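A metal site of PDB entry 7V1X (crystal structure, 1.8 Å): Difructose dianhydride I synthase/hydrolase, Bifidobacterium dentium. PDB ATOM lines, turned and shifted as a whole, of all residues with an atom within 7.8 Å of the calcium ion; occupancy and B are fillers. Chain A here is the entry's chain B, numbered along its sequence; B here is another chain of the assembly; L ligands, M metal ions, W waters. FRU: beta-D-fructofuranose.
O1 of the ligand sits at hydrogen-bond distance from OE2 of Glu 270, at 2.5 Å.
The backbone carbonyl oxygen (O) of Thr 288 lies close to an oxygen (O4) of the ligand, at 3.4 Å.
O3 of the ligand is in hydrogen-bond range of O of Gly 269, at 3.3 Å.
O6 of the ligand sits at hydrogen-bond distance from OD1 of Asp 292 (2.6 Å).
OE2 of Glu 291 sits at hydrogen-bond distance from O2 of the ligand, at 2.5 Å.
The backbone NH of Asn 31 of chain B lies within hydrogen-bond range of the side-chain carboxylate of Asp 26 of chain B.
ND2 of Asn 31 of chain B is in hydrogen-bond range of OD1 of Asn 231, 3.0 Å away.
ND2 of Asn 31 of chain B lies within hydrogen-bond range of OD1 of Asn 226, at 3.3 Å.
N of Gly 289 lies close to OD1 of Asn 272, 3.4 Å away.
The backbone NH of Asn 272 is in hydrogen-bond range of the side-chain carboxylate of Glu 343, at 2.8 Å.
The side-chain amide nitrogen (ND2) of Asn 272 lies within hydrogen-bond range of the backbone carbonyl oxygen (O) of Gly 287 (3.0 Å).
OE2 of Glu 270 sits at hydrogen-bond distance from ND2 of Asn 226, at 2.9 Å.
OD2 of Asp 292 sits at hydrogen-bond distance from OG1 of Thr 288.
Five residues have an atom within 4 Å of the calcium ion: Glu 270, Asn 272, Thr 288, Asn 31 of chain B and Asp 33 of chain B.
The nearest printed residue that does not touch the calcium ion is Gly 289 (4.2 Å).
OD2 of Asp 33 of chain B binds the calcium ion (2.3 Å).
The calcium ion is bound by OD1 of Asn 31 of chain B, 2.4 Å away.
The side-chain amide oxygen (OD1) of Asn 272 binds the calcium ion (2.4 Å).
The backbone carbonyl oxygen (O) of Glu 270 is bound to the calcium ion (2.4 Å).
The calcium ion is bound by water W1 (2.5 Å).
The calcium ion is bound by water W2.
The calcium ion is bound by O of Thr 288, at 2.6 Å.
Water W2 bridges the side-chain carboxylate of Glu 343 (2.7 Å) and a ring nitrogen (ND1) of His 346 (2.8 Å).
Water W1 lies within hydrogen-bond range of the side-chain carboxylate (OE1) of Glu 270 (2.6 Å) and an oxygen (O4) of the ligand (2.8 Å).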
ATOM      1  N   ASN A 226      16.196  14.427  -2.509  1.00  0.00           N
ATOM      2  CA  ASN A 226      16.138  14.754  -3.962  1.00  0.00           C
ATOM      3  C   ASN A 226      15.999  13.492  -4.792  1.00  0.00           C
ATOM      4  O   ASN A 226      16.186  13.566  -6.020  1.00  0.00           O
ATOM      5  CB  ASN A 226      17.364  15.543  -4.404  1.00  0.00           C
ATOM      6  CG  ASN A 226      17.241  16.992  -4.018  1.00  0.00           C
ATOM      7  OD1 ASN A 226      16.125  17.526  -3.966  1.00  0.00           O
ATOM      8  ND2 ASN A 226      18.369  17.636  -3.733  1.00  0.00           N
ATOM      9  N   ASN A 231      10.805  14.247  -4.173  1.00  0.00           N
ATOM     10  CA  ASN A 231      10.552  15.536  -4.875  1.00  0.00           C
ATOM     11  C   ASN A 231       9.133  15.604  -5.426  1.00  0.00           C
ATOM     12  O   ASN A 231       8.654  16.739  -5.661  1.00  0.00           O
ATOM     13  CB  ASN A 231      11.608  15.762  -5.954  1.00  0.00           C
ATOM     14  CG  ASN A 231      12.921  16.236  -5.375  1.00  0.00           C
ATOM     15  OD1 ASN A 231      12.977  16.680  -4.226  1.00  0.00           O
ATOM     16  ND2 ASN A 231      13.962  16.219  -6.177  1.00  0.00           N
ATOM     17  N   GLY A 269      18.541  21.398   2.963  1.00  0.00           N
ATOM     18  CA  GLY A 269      18.023  22.745   2.647  1.00  0.00           C
ATOM     19  C   GLY A 269      17.067  22.846   1.464  1.00  0.00           C
ATOM     20  O   GLY A 269      16.889  23.969   0.974  1.00  0.00           O
ATOM     21  N   GLU A 270      16.343  21.790   1.075  1.00  0.00           N
ATOM     22  CA  GLU A 270      15.414  21.929  -0.086  1.00  0.00           C
ATOM     23  C   GLU A 270      14.134  22.673   0.327  1.00  0.00           C
ATOM     24  O   GLU A 270      13.417  23.087  -0.545  1.00  0.00           O
ATOM     25  CB  GLU A 270      15.080  20.548  -0.639  1.00  0.00           C
ATOM     26  CG  GLU A 270      16.234  19.895  -1.322  1.00  0.00           C
ATOM     27  CD  GLU A 270      16.672  20.542  -2.610  1.00  0.00           C
ATOM     28  OE1 GLU A 270      15.852  21.234  -3.239  1.00  0.00           O
ATOM     29  OE2 GLU A 270      17.848  20.362  -2.974  1.00  0.00           O
ATOM     30  N   GLY A 271      13.843  22.815   1.616  1.00  0.00           N
ATOM     31  CA  GLY A 271      12.544  23.283   2.093  1.00  0.00           C
ATOM     32  C   GLY A 271      12.370  24.758   1.848  1.00  0.00           C
ATOM     33  O   GLY A 271      13.381  25.515   1.862  1.00  0.00           O
ATOM     34  N   ASN A 272      11.158  25.114   1.456  1.00  0.00           N
ATOM     35  CA  ASN A 272      10.788  26.499   1.088  1.00  0.00           C
ATOM     36  C   ASN A 272      10.436  27.272   2.350  1.00  0.00           C
ATOM     37  O   ASN A 272       9.691  26.750   3.177  1.00  0.00           O
ATOM     38  CB  ASN A 272       9.615  26.514   0.115  1.00  0.00           C
ATOM     39  CG  ASN A 272       9.890  25.944  -1.261  1.00  0.00           C
ATOM     40  OD1 ASN A 272      10.977  25.411  -1.564  1.00  0.00           O
ATOM     41  ND2 ASN A 272       8.839  25.933  -2.080  1.00  0.00           N
ATOM     42  N   ASP A 273      10.899  28.512   2.451  1.00  0.00           N
ATOM     43  CA  ASP A 273      10.232  29.524   3.311  1.00  0.00           C
ATOM     44  C   ASP A 273       8.792  29.734   2.824  1.00  0.00           C
ATOM     45  O   ASP A 273       8.513  29.813   1.607  1.00  0.00           O
ATOM     46  CB  ASP A 273      11.043  30.815   3.380  1.00  0.00           C
ATOM     47  CG  ASP A 273      11.340  31.439   2.030  1.00  0.00           C
ATOM     48  OD1 ASP A 273      12.076  30.792   1.213  1.00  0.00           O
ATOM     49  OD2 ASP A 273      10.826  32.557   1.814  1.00  0.00           O
ATOM     50  N   MET A 274       7.877  29.808   3.785  1.00  0.00           N
ATOM     51  CA  MET A 274       6.438  30.074   3.559  1.00  0.00           C
ATOM     52  C   MET A 274       6.008  30.996   4.680  1.00  0.00           C
ATOM     53  O   MET A 274       6.121  30.625   5.863  1.00  0.00           O
ATOM     54  CB  MET A 274       5.605  28.791   3.559  1.00  0.00           C
ATOM     55  CG  MET A 274       5.975  27.837   2.455  1.00  0.00           C
ATOM     56  SD  MET A 274       4.844  26.434   2.345  1.00  0.00           S
ATOM     57  CE  MET A 274       5.704  25.395   1.177  1.00  0.00           C
ATOM     58  N   GLY A 287       8.701  30.762  -1.037  1.00  0.00           N
ATOM     59  CA  GLY A 287      10.112  30.730  -1.469  1.00  0.00           C
ATOM     60  C   GLY A 287      10.395  29.442  -2.165  1.00  0.00           C
ATOM     61  O   GLY A 287       9.468  28.798  -2.665  1.00  0.00           O
ATOM     62  N   THR A 288      11.669  29.120  -2.315  1.00  0.00           N
ATOM     63  CA  THR A 288      12.093  28.084  -3.248  1.00  0.00           C
ATOM     64  C   THR A 288      13.008  27.076  -2.585  1.00  0.00           C
ATOM     65  O   THR A 288      13.162  25.984  -3.115  1.00  0.00           O
ATOM     66  CB  THR A 288      12.685  28.776  -4.487  1.00  0.00           C
ATOM     67  OG1 THR A 288      13.761  29.583  -4.013  1.00  0.00           O
ATOM     68  CG2 THR A 288      11.652  29.613  -5.198  1.00  0.00           C
ATOM     69  N   GLY A 289      13.667  27.449  -1.504  1.00  0.00           N
ATOM     70  CA  GLY A 289      14.671  26.558  -0.900  1.00  0.00           C
ATOM     71  C   GLY A 289      15.254  27.220   0.320  1.00  0.00           C
ATOM     72  O   GLY A 289      15.039  28.443   0.492  1.00  0.00           O
ATOM     73  N   THR A 290      15.961  26.495   1.167  1.00  0.00           N
ATOM     74  CA  THR A 290      16.378  27.125   2.451  1.00  0.00           C
ATOM     75  C   THR A 290      17.641  27.985   2.237  1.00  0.00           C
ATOM     76  O   THR A 290      17.685  29.100   2.786  1.00  0.00           O
ATOM     77  CB  THR A 290      16.566  26.057   3.522  1.00  0.00           C
ATOM     78  OG1 THR A 290      15.374  25.255   3.599  1.00  0.00           O
ATOM     79  CG2 THR A 290      16.848  26.682   4.864  1.00  0.00           C
ATOM     80  N   GLU A 291      18.618  27.524   1.444  1.00  0.00           N
ATOM     81  CA  GLU A 291      19.780  28.388   1.128  1.00  0.00           C
ATOM     82  C   GLU A 291      19.258  29.585   0.326  1.00  0.00           C
ATOM     83  O   GLU A 291      19.771  30.718   0.528  1.00  0.00           O
ATOM     84  CB  GLU A 291      20.904  27.646   0.423  1.00  0.00           C
ATOM     85  CG  GLU A 291      20.770  27.474  -1.076  1.00  0.00           C
ATOM     86  CD  GLU A 291      20.078  26.191  -1.440  1.00  0.00           C
ATOM     87  OE1 GLU A 291      18.955  25.993  -0.901  1.00  0.00           O
ATOM     88  OE2 GLU A 291      20.657  25.340  -2.200  1.00  0.00           O
ATOM     89  N   ASP A 292      18.219  29.350  -0.491  1.00  0.00           N
ATOM     90  CA  ASP A 292      17.628  30.438  -1.318  1.00  0.00           C
ATOM     91  C   ASP A 292      17.079  31.519  -0.399  1.00  0.00           C
ATOM     92  O   ASP A 292      17.259  32.728  -0.714  1.00  0.00           O
ATOM     93  CB  ASP A 292      16.572  29.906  -2.275  1.00  0.00           C
ATOM     94  CG  ASP A 292      16.982  28.688  -3.104  1.00  0.00           C
ATOM     95  OD1 ASP A 292      18.189  28.337  -3.153  1.00  0.00           O
ATOM     96  OD2 ASP A 292      16.067  28.130  -3.777  1.00  0.00           O
ATOM     97  N   GLU A 343       9.835  24.686   5.295  1.00  0.00           N
ATOM     98  CA  GLU A 343       9.741  23.217   5.195  1.00  0.00           C
ATOM     99  C   GLU A 343      11.045  22.652   5.717  1.00  0.00           C
ATOM    100  O   GLU A 343      12.146  23.130   5.316  1.00  0.00           O
ATOM    101  CB  GLU A 343       9.514  22.773   3.767  1.00  0.00           C
ATOM    102  CG  GLU A 343       8.367  23.472   3.035  1.00  0.00           C
ATOM    103  CD  GLU A 343       8.294  22.909   1.640  1.00  0.00           C
ATOM    104  OE1 GLU A 343       9.219  23.203   0.809  1.00  0.00           O
ATOM    105  OE2 GLU A 343       7.386  22.078   1.375  1.00  0.00           O
ATOM    106  N   GLY A 345      13.396  20.190   5.125  1.00  0.00           N
ATOM    107  CA  GLY A 345      13.512  19.430   3.883  1.00  0.00           C
ATOM    108  C   GLY A 345      12.310  19.670   3.013  1.00  0.00           C
ATOM    109  O   GLY A 345      11.292  20.208   3.508  1.00  0.00           O
ATOM    110  N   HIS A 346      12.390  19.249   1.749  1.00  0.00           N
ATOM    111  CA  HIS A 346      11.230  19.342   0.838  1.00  0.00           C
ATOM    112  C   HIS A 346       9.998  18.696   1.488  1.00  0.00           C
ATOM    113  O   HIS A 346      10.066  17.524   1.869  1.00  0.00           O
ATOM    114  CB  HIS A 346      11.498  18.690  -0.500  1.00  0.00           C
ATOM    115  CG  HIS A 346      10.224  18.676  -1.255  1.00  0.00           C
ATOM    116  ND1 HIS A 346       9.522  19.874  -1.506  1.00  0.00           N
ATOM    117  CD2 HIS A 346       9.459  17.660  -1.684  1.00  0.00           C
ATOM    118  CE1 HIS A 346       8.411  19.563  -2.142  1.00  0.00           C
ATOM    119  NE2 HIS A 346       8.348  18.223  -2.244  1.00  0.00           N
ATOM    120  N   ALA A 347       8.900  19.418   1.535  1.00  0.00           N
ATOM    121  CA  ALA A 347       7.614  18.877   2.048  1.00  0.00           C
ATOM    122  C   ALA A 347       7.814  18.228   3.433  1.00  0.00           C
ATOM    123  O   ALA A 347       7.133  17.282   3.756  1.00  0.00           O
ATOM    124  CB  ALA A 347       7.035  17.910   1.038  1.00  0.00           C
ATOM    125  N   TRP B  25       8.442  29.506  -7.238  1.00  0.00           N
ATOM    126  CA  TRP B  25       7.969  28.419  -6.372  1.00  0.00           C
ATOM    127  C   TRP B  25       7.107  27.435  -7.174  1.00  0.00           C
ATOM    128  O   TRP B  25       6.427  27.852  -8.143  1.00  0.00           O
ATOM    129  CB  TRP B  25       7.221  28.931  -5.161  1.00  0.00           C
ATOM    130  CG  TRP B  25       5.877  29.534  -5.411  1.00  0.00           C
ATOM    131  CD1 TRP B  25       5.589  30.788  -5.880  1.00  0.00           C
ATOM    132  CD2 TRP B  25       4.615  28.925  -5.085  1.00  0.00           C
ATOM    133  NE1 TRP B  25       4.231  30.991  -5.882  1.00  0.00           N
ATOM    134  CE2 TRP B  25       3.612  29.862  -5.398  1.00  0.00           C
ATOM    135  CE3 TRP B  25       4.239  27.675  -4.587  1.00  0.00           C
ATOM    136  CZ2 TRP B  25       2.255  29.584  -5.228  1.00  0.00           C
ATOM    137  CZ3 TRP B  25       2.895  27.388  -4.451  1.00  0.00           C
ATOM    138  CH2 TRP B  25       1.927  28.332  -4.769  1.00  0.00           C
ATOM    139  N   ASP B  26       7.237  26.161  -6.834  1.00  0.00           N
ATOM    140  CA  ASP B  26       6.607  25.054  -7.588  1.00  0.00           C
ATOM    141  C   ASP B  26       5.111  25.061  -7.277  1.00  0.00           C
ATOM    142  O   ASP B  26       4.738  24.738  -6.129  1.00  0.00           O
ATOM    143  CB  ASP B  26       7.286  23.744  -7.214  1.00  0.00           C
ATOM    144  CG  ASP B  26       6.829  22.587  -8.071  1.00  0.00           C
ATOM    145  OD1 ASP B  26       5.693  22.663  -8.631  1.00  0.00           O
ATOM    146  OD2 ASP B  26       7.564  21.585  -8.087  1.00  0.00           O
ATOM    147  N   LYS B  30       5.469  20.810  -5.348  1.00  0.00           N
ATOM    148  CA  LYS B  30       6.526  19.795  -5.360  1.00  0.00           C
ATOM    149  C   LYS B  30       7.865  20.558  -5.208  1.00  0.00           C
ATOM    150  O   LYS B  30       7.832  21.692  -4.745  1.00  0.00           O
ATOM    151  CB  LYS B  30       6.399  18.912  -6.600  1.00  0.00           C
ATOM    152  CG  LYS B  30       5.146  18.062  -6.606  1.00  0.00           C
ATOM    153  CD  LYS B  30       4.939  17.333  -7.894  1.00  0.00           C
ATOM    154  CE  LYS B  30       3.528  16.801  -8.040  1.00  0.00           C
ATOM    155  NZ  LYS B  30       3.579  15.378  -8.413  1.00  0.00           N
ATOM    156  N   ASN B  31       8.966  19.961  -5.600  1.00  0.00           N
ATOM    157  CA  ASN B  31      10.315  20.528  -5.333  1.00  0.00           C
ATOM    158  C   ASN B  31      11.027  20.956  -6.623  1.00  0.00           C
ATOM    159  O   ASN B  31      12.239  20.967  -6.641  1.00  0.00           O
ATOM    160  CB  ASN B  31      11.179  19.568  -4.534  1.00  0.00           C
ATOM    161  CG  ASN B  31      12.364  20.274  -3.904  1.00  0.00           C
ATOM    162  OD1 ASN B  31      12.227  21.395  -3.459  1.00  0.00           O
ATOM    163  ND2 ASN B  31      13.522  19.610  -3.870  1.00  0.00           N
ATOM    164  N   GLN B  32      10.297  21.390  -7.646  1.00  0.00           N
ATOM    165  CA  GLN B  32      10.895  22.088  -8.800  1.00  0.00           C
ATOM    166  C   GLN B  32      10.575  23.574  -8.669  1.00  0.00           C
ATOM    167  O   GLN B  32       9.783  24.069  -9.459  1.00  0.00           O
ATOM    168  CB  GLN B  32      10.329  21.589 -10.124  1.00  0.00           C
ATOM    169  CG  GLN B  32      10.850  20.263 -10.547  1.00  0.00           C
ATOM    170  CD  GLN B  32      10.254  19.839 -11.876  1.00  0.00           C
ATOM    171  OE1 GLN B  32       9.796  20.648 -12.694  1.00  0.00           O
ATOM    172  NE2 GLN B  32      10.278  18.542 -12.085  1.00  0.00           N
ATOM    173  N   ASP B  33      11.199  24.251  -7.694  1.00  0.00           N
ATOM    174  CA  ASP B  33      10.912  25.663  -7.337  1.00  0.00           C
ATOM    175  C   ASP B  33      11.705  26.609  -8.274  1.00  0.00           C
ATOM    176  O   ASP B  33      12.182  27.677  -7.831  1.00  0.00           O
ATOM    177  CB  ASP B  33      11.156  25.900  -5.836  1.00  0.00           C
ATOM    178  CG  ASP B  33      10.347  25.001  -4.923  1.00  0.00           C
ATOM    179  OD1 ASP B  33       9.138  25.210  -4.826  1.00  0.00           O
ATOM    180  OD2 ASP B  33      10.914  24.010  -4.465  1.00  0.00           O
ATOM    181  N   TYR B  34      11.801  26.252  -9.553  1.00  0.00           N
ATOM    182  CA  TYR B  34      12.531  26.995 -10.589  1.00  0.00           C
ATOM    183  C   TYR B  34      11.683  26.940 -11.863  1.00  0.00           C
ATOM    184  O   TYR B  34      10.787  26.058 -11.968  1.00  0.00           O
ATOM    185  CB  TYR B  34      13.905  26.383 -10.819  1.00  0.00           C
ATOM    186  CG  TYR B  34      13.885  24.951 -11.276  1.00  0.00           C
ATOM    187  CD1 TYR B  34      13.846  24.613 -12.619  1.00  0.00           C
ATOM    188  CD2 TYR B  34      13.978  23.916 -10.357  1.00  0.00           C
ATOM    189  CE1 TYR B  34      13.879  23.288 -13.025  1.00  0.00           C
ATOM    190  CE2 TYR B  34      13.929  22.594 -10.750  1.00  0.00           C
ATOM    191  CZ  TYR B  34      13.921  22.273 -12.083  1.00  0.00           C
ATOM    192  OH  TYR B  34      13.940  20.958 -12.441  1.00  0.00           O
ATOM    193  N   TYR B 187      15.822  30.301 -10.820  1.00  0.00           N
ATOM    194  CA  TYR B 187      15.184  30.423  -9.492  1.00  0.00           C
ATOM    195  C   TYR B 187      15.111  31.926  -9.238  1.00  0.00           C
ATOM    196  O   TYR B 187      16.101  32.655  -9.488  1.00  0.00           O
ATOM    197  CB  TYR B 187      16.036  29.794  -8.393  1.00  0.00           C
ATOM    198  CG  TYR B 187      16.059  28.291  -8.254  1.00  0.00           C
ATOM    199  CD1 TYR B 187      16.897  27.476  -8.998  1.00  0.00           C
ATOM    200  CD2 TYR B 187      15.239  27.698  -7.310  1.00  0.00           C
ATOM    201  CE1 TYR B 187      16.900  26.084  -8.815  1.00  0.00           C
ATOM    202  CE2 TYR B 187      15.216  26.322  -7.123  1.00  0.00           C
ATOM    203  CZ  TYR B 187      16.049  25.505  -7.874  1.00  0.00           C
ATOM    204  OH  TYR B 187      16.032  24.161  -7.673  1.00  0.00           O
HETATM  205  C1  FRU L   1      19.296  22.369  -5.378  1.00  0.00           C
HETATM  206  C2  FRU L   1      19.474  23.440  -4.275  1.00  0.00           C
HETATM  207  C3  FRU L   1      18.152  23.734  -3.516  1.00  0.00           C
HETATM  208  C4  FRU L   1      17.822  25.152  -4.002  1.00  0.00           C
HETATM  209  C5  FRU L   1      18.517  25.277  -5.340  1.00  0.00           C
HETATM  210  C6  FRU L   1      18.832  26.677  -5.848  1.00  0.00           C
HETATM  211  O1  FRU L   1      19.280  21.023  -4.849  1.00  0.00           O
HETATM  212  O2  FRU L   1      20.560  23.125  -3.384  1.00  0.00           O
HETATM  213  O3  FRU L   1      18.046  23.729  -2.069  1.00  0.00           O
HETATM  214  O4  FRU L   1      16.397  25.491  -4.073  1.00  0.00           O
HETATM  215  O5  FRU L   1      19.730  24.628  -5.066  1.00  0.00           O
HETATM  216  O6  FRU L   1      19.715  27.404  -4.978  1.00  0.00           O
HETATM  217 CA    CA M   1      12.210  23.621  -2.578  1.00  0.00          CA
HETATM  218  O   HOH W   1      14.509  23.440  -3.566  1.00  0.00           O
HETATM  219  O   HOH W   2      10.109  22.590  -1.671  1.00  0.00           O
